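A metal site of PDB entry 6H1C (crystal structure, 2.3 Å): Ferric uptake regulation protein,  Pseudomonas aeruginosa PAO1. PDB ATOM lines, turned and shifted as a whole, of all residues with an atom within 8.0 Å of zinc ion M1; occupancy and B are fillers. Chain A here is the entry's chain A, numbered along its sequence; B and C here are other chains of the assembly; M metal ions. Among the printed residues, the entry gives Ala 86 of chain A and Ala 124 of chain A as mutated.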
ATOM      1  N   VAL A  68     -23.404  13.811  10.735  1.00  0.00           N
ATOM      2  CA  VAL A  68     -22.733  12.987   9.736  1.00  0.00           C
ATOM      3  C   VAL A  68     -21.236  12.987   9.997  1.00  0.00           C
ATOM      4  O   VAL A  68     -20.649  14.032  10.263  1.00  0.00           O
ATOM      5  CB  VAL A  68     -23.017  13.499   8.310  1.00  0.00           C
ATOM      6  CG1 VAL A  68     -22.219  12.687   7.293  1.00  0.00           C
ATOM      7  CG2 VAL A  68     -24.483  13.445   7.994  1.00  0.00           C
ATOM      8  N   ARG A  69     -20.621  11.825   9.874  1.00  0.00           N
ATOM      9  CA  ARG A  69     -19.195  11.631  10.118  1.00  0.00           C
ATOM     10  C   ARG A  69     -18.489  11.366   8.800  1.00  0.00           C
ATOM     11  O   ARG A  69     -18.857  10.434   8.084  1.00  0.00           O
ATOM     12  CB  ARG A  69     -18.994  10.450  11.077  1.00  0.00           C
ATOM     13  CG  ARG A  69     -17.561  10.165  11.495  1.00  0.00           C
ATOM     14  CD  ARG A  69     -17.477   8.789  12.218  1.00  0.00           C
ATOM     15  NE  ARG A  69     -16.190   8.573  12.872  1.00  0.00           N
ATOM     16  CZ  ARG A  69     -16.010   8.431  14.187  1.00  0.00           C
ATOM     17  NH1 ARG A  69     -17.040   8.463  15.041  1.00  0.00           N
ATOM     18  NH2 ARG A  69     -14.787   8.236  14.665  1.00  0.00           N
ATOM     19  N   HIS A  70     -17.475  12.151   8.478  1.00  0.00           N
ATOM     20  CA  HIS A  70     -16.654  11.890   7.313  1.00  0.00           C
ATOM     21  C   HIS A  70     -15.203  11.737   7.748  1.00  0.00           C
ATOM     22  O   HIS A  70     -14.823  12.174   8.824  1.00  0.00           O
ATOM     23  CB  HIS A  70     -16.733  13.016   6.263  1.00  0.00           C
ATOM     24  CG  HIS A  70     -18.121  13.356   5.814  1.00  0.00           C
ATOM     25  ND1 HIS A  70     -18.894  12.489   5.070  1.00  0.00           N
ATOM     26  CD2 HIS A  70     -18.864  14.482   5.973  1.00  0.00           C
ATOM     27  CE1 HIS A  70     -20.052  13.057   4.801  1.00  0.00           C
ATOM     28  NE2 HIS A  70     -20.062  14.266   5.338  1.00  0.00           N
ATOM     29  N   ALA A  82     -26.266  17.037  10.181  1.00  0.00           N
ATOM     30  CA  ALA A  82     -26.930  16.320   9.088  1.00  0.00           C
ATOM     31  C   ALA A  82     -27.975  17.216   8.409  1.00  0.00           C
ATOM     32  O   ALA A  82     -29.184  17.056   8.561  1.00  0.00           O
ATOM     33  CB  ALA A  82     -27.570  15.032   9.594  1.00  0.00           C
ATOM     34  N   ASP A  83     -27.476  18.171   7.631  1.00  0.00           N
ATOM     35  CA  ASP A  83     -28.316  19.065   6.859  1.00  0.00           C
ATOM     36  C   ASP A  83     -28.233  18.722   5.376  1.00  0.00           C
ATOM     37  O   ASP A  83     -27.541  17.779   4.961  1.00  0.00           O
ATOM     38  CB  ASP A  83     -27.923  20.527   7.123  1.00  0.00           C
ATOM     39  CG  ASP A  83     -26.475  20.821   6.803  1.00  0.00           C
ATOM     40  OD1 ASP A  83     -25.933  20.214   5.846  1.00  0.00           O
ATOM     41  OD2 ASP A  83     -25.866  21.665   7.497  1.00  0.00           O
ATOM     42  N   GLY A  85     -26.607  19.285   2.048  1.00  0.00           N
ATOM     43  CA  GLY A  85     -25.248  19.673   1.770  1.00  0.00           C
ATOM     44  C   GLY A  85     -24.211  18.818   2.461  1.00  0.00           C
ATOM     45  O   GLY A  85     -23.045  18.843   2.063  1.00  0.00           O
ATOM     46  N   ALA A  86     -24.610  18.033   3.464  1.00  0.00           N
ATOM     47  CA  ALA A  86     -23.669  17.252   4.247  1.00  0.00           C
ATOM     48  C   ALA A  86     -23.252  15.931   3.605  1.00  0.00           C
ATOM     49  O   ALA A  86     -22.500  15.182   4.232  1.00  0.00           O
ATOM     50  CB  ALA A  86     -24.265  16.964   5.625  1.00  0.00           C
ATOM     51  N   HIS A  87     -23.723  15.616   2.393  1.00  0.00           N
ATOM     52  CA  HIS A  87     -23.386  14.359   1.731  1.00  0.00           C
ATOM     53  C   HIS A  87     -22.686  14.542   0.400  1.00  0.00           C
ATOM     54  O   HIS A  87     -22.380  13.546  -0.264  1.00  0.00           O
ATOM     55  CB  HIS A  87     -24.624  13.504   1.510  1.00  0.00           C
ATOM     56  CG  HIS A  87     -25.691  13.690   2.537  1.00  0.00           C
ATOM     57  ND1 HIS A  87     -25.842  12.848   3.620  1.00  0.00           N
ATOM     58  CD2 HIS A  87     -26.684  14.610   2.640  1.00  0.00           C
ATOM     59  CE1 HIS A  87     -26.874  13.244   4.346  1.00  0.00           C
ATOM     60  NE2 HIS A  87     -27.401  14.322   3.785  1.00  0.00           N
ATOM     61  N   ASP A  88     -22.435  15.775  -0.034  1.00  0.00           N
ATOM     62  CA  ASP A  88     -21.799  16.071  -1.313  1.00  0.00           C
ATOM     63  C   ASP A  88     -20.617  16.999  -1.064  1.00  0.00           C
ATOM     64  O   ASP A  88     -20.806  18.137  -0.640  1.00  0.00           O
ATOM     65  CB  ASP A  88     -22.796  16.724  -2.291  1.00  0.00           C
ATOM     66  CG  ASP A  88     -23.776  15.740  -2.878  1.00  0.00           C
ATOM     67  OD1 ASP A  88     -23.413  15.084  -3.876  1.00  0.00           O
ATOM     68  OD2 ASP A  88     -24.905  15.603  -2.359  1.00  0.00           O
ATOM     69  N   HIS A  89     -19.398  16.519  -1.326  1.00  0.00           N
ATOM     70  CA  HIS A  89     -18.177  17.264  -1.041  1.00  0.00           C
ATOM     71  C   HIS A  89     -17.169  17.059  -2.156  1.00  0.00           C
ATOM     72  O   HIS A  89     -17.018  15.948  -2.656  1.00  0.00           O
ATOM     73  CB  HIS A  89     -17.532  16.838   0.295  1.00  0.00           C
ATOM     74  CG  HIS A  89     -18.312  17.227   1.506  1.00  0.00           C
ATOM     75  ND1 HIS A  89     -19.274  16.427   2.074  1.00  0.00           N
ATOM     76  CD2 HIS A  89     -18.279  18.356   2.266  1.00  0.00           C
ATOM     77  CE1 HIS A  89     -19.787  17.026   3.129  1.00  0.00           C
ATOM     78  NE2 HIS A  89     -19.212  18.202   3.263  1.00  0.00           N
ATOM     79  N   VAL A 122     -32.405   5.769   0.443  1.00  0.00           N
ATOM     80  CA  VAL A 122     -32.355   6.180   1.840  1.00  0.00           C
ATOM     81  C   VAL A 122     -31.315   7.263   2.058  1.00  0.00           C
ATOM     82  O   VAL A 122     -31.492   8.134   2.896  1.00  0.00           O
ATOM     83  CB  VAL A 122     -32.094   4.972   2.743  1.00  0.00           C
ATOM     84  CG1 VAL A 122     -32.249   5.375   4.194  1.00  0.00           C
ATOM     85  CG2 VAL A 122     -33.025   3.819   2.403  1.00  0.00           C
ATOM     86  N   ASP A 123     -30.204   7.223   1.338  1.00  0.00           N
ATOM     87  CA  ASP A 123     -29.125   8.172   1.505  1.00  0.00           C
ATOM     88  C   ASP A 123     -28.092   7.926   0.416  1.00  0.00           C
ATOM     89  O   ASP A 123     -27.908   6.804  -0.036  1.00  0.00           O
ATOM     90  CB  ASP A 123     -28.476   8.055   2.880  1.00  0.00           C
ATOM     91  CG  ASP A 123     -27.793   9.347   3.305  1.00  0.00           C
ATOM     92  OD1 ASP A 123     -26.692   9.658   2.788  1.00  0.00           O
ATOM     93  OD2 ASP A 123     -28.377  10.056   4.151  1.00  0.00           O
ATOM     94  N   ALA A 124     -27.424   9.002   0.016  1.00  0.00           N
ATOM     95  CA  ALA A 124     -26.409   8.959  -1.019  1.00  0.00           C
ATOM     96  C   ALA A 124     -25.192   9.739  -0.541  1.00  0.00           C
ATOM     97  O   ALA A 124     -25.322  10.713   0.201  1.00  0.00           O
ATOM     98  CB  ALA A 124     -26.929   9.554  -2.343  1.00  0.00           C
ATOM     99  N   ASN A 125     -24.009   9.298  -0.938  1.00  0.00           N
ATOM    100  CA  ASN A 125     -22.797  10.025  -0.623  1.00  0.00           C
ATOM    101  C   ASN A 125     -21.903  10.137  -1.841  1.00  0.00           C
ATOM    102  O   ASN A 125     -21.616   9.130  -2.495  1.00  0.00           O
ATOM    103  CB  ASN A 125     -22.036   9.369   0.520  1.00  0.00           C
ATOM    104  CG  ASN A 125     -22.709   9.613   1.836  1.00  0.00           C
ATOM    105  OD1 ASN A 125     -23.306  10.678   2.042  1.00  0.00           O
ATOM    106  ND2 ASN A 125     -22.627   8.644   2.725  1.00  0.00           N
ATOM    107  N   LEU A 126     -21.469  11.366  -2.116  1.00  0.00           N
ATOM    108  CA  LEU A 126     -20.607  11.654  -3.251  1.00  0.00           C
ATOM    109  C   LEU A 126     -19.361  12.367  -2.759  1.00  0.00           C
ATOM    110  O   LEU A 126     -19.451  13.350  -2.029  1.00  0.00           O
ATOM    111  CB  LEU A 126     -21.372  12.502  -4.272  1.00  0.00           C
ATOM    112  CG  LEU A 126     -20.702  12.753  -5.627  1.00  0.00           C
ATOM    113  CD1 LEU A 126     -20.250  11.443  -6.240  1.00  0.00           C
ATOM    114  CD2 LEU A 126     -21.633  13.482  -6.564  1.00  0.00           C
ATOM    115  N   VAL B 127     -21.924   6.322  -3.199  1.00  0.00           N
ATOM    116  CA  VAL B 127     -22.576   5.207  -2.521  1.00  0.00           C
ATOM    117  C   VAL B 127     -24.032   5.557  -2.321  1.00  0.00           C
ATOM    118  O   VAL B 127     -24.349   6.610  -1.783  1.00  0.00           O
ATOM    119  CB  VAL B 127     -21.912   4.864  -1.180  1.00  0.00           C
ATOM    120  CG1 VAL B 127     -22.709   3.761  -0.472  1.00  0.00           C
ATOM    121  CG2 VAL B 127     -20.471   4.405  -1.416  1.00  0.00           C
ATOM    122  N   TYR B 129     -27.375   4.276  -0.579  1.00  0.00           N
ATOM    123  CA  TYR B 129     -28.025   3.407   0.395  1.00  0.00           C
ATOM    124  C   TYR B 129     -29.503   3.336   0.069  1.00  0.00           C
ATOM    125  O   TYR B 129     -30.180   4.362   0.006  1.00  0.00           O
ATOM    126  CB  TYR B 129     -27.808   3.923   1.818  1.00  0.00           C
ATOM    127  CG  TYR B 129     -26.347   3.980   2.176  1.00  0.00           C
ATOM    128  CD1 TYR B 129     -25.664   2.825   2.541  1.00  0.00           C
ATOM    129  CD2 TYR B 129     -25.640   5.168   2.131  1.00  0.00           C
ATOM    130  CE1 TYR B 129     -24.322   2.854   2.864  1.00  0.00           C
ATOM    131  CE2 TYR B 129     -24.305   5.201   2.465  1.00  0.00           C
ATOM    132  CZ  TYR B 129     -23.650   4.041   2.822  1.00  0.00           C
ATOM    133  OH  TYR B 129     -22.305   4.056   3.144  1.00  0.00           O
ATOM    134  N   ARG C  56     -26.125   0.849  13.968  1.00  0.00           N
ATOM    135  CA  ARG C  56     -26.341   2.120  14.663  1.00  0.00           C
ATOM    136  C   ARG C  56     -26.588   1.888  16.141  1.00  0.00           C
ATOM    137  O   ARG C  56     -26.097   2.639  16.988  1.00  0.00           O
ATOM    138  CB  ARG C  56     -27.495   2.896  14.045  1.00  0.00           C
ATOM    139  CG  ARG C  56     -27.098   3.543  12.753  1.00  0.00           C
ATOM    140  CD  ARG C  56     -28.235   4.331  12.114  1.00  0.00           C
ATOM    141  NE  ARG C  56     -27.799   4.820  10.810  1.00  0.00           N
ATOM    142  CZ  ARG C  56     -27.084   5.933  10.619  1.00  0.00           C
ATOM    143  NH1 ARG C  56     -26.730   6.701  11.657  1.00  0.00           N
ATOM    144  NH2 ARG C  56     -26.712   6.295   9.391  1.00  0.00           N
HETATM  145 ZN    ZN M   1     -24.810  11.143   3.667  1.00  0.00          ZN
HETATM  146 ZN    ZN M   2     -26.348  10.109   5.906  1.00  0.00          ZN
HETATM  147 MN    MN M   3     -18.413  10.966   3.910  1.00  0.00          MN
HETATM  148 MN    MN M   4     -26.442  14.514  -2.573  1.00  0.00          MN
HETATM  149 MN    MN M   5     -16.899  10.527   3.902  1.00  0.00          MN
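O of Val 127 of chain B sits at hydrogen-bond distance from N of Asn 125.
The backbone NH of Leu 126 sits at hydrogen-bond distance from the backbone carbonyl oxygen of His 87.
The backbone NH (N) of Tyr 129 of chain B is in hydrogen-bond range of the backbone carbonyl oxygen (O) of Asp 123 (2.6 Å).
Residues that only touch zinc ion M1: Ala 124 (3.5 Å).
Four residues have an atom within 4 Å of zinc ion M1: His 87, Asp 123, Ala 124 and Asn 125.
The nearest printed residue that does not touch zinc ion M1 is Ala 86 (4.7 Å).
ND1 of His 87 binds zinc ion M1, at 2.0 Å.
OD1 of Asn 125 binds zinc ion M1 (2.3 Å).
OD1 of Asp 123 is bound to zinc ion M1.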
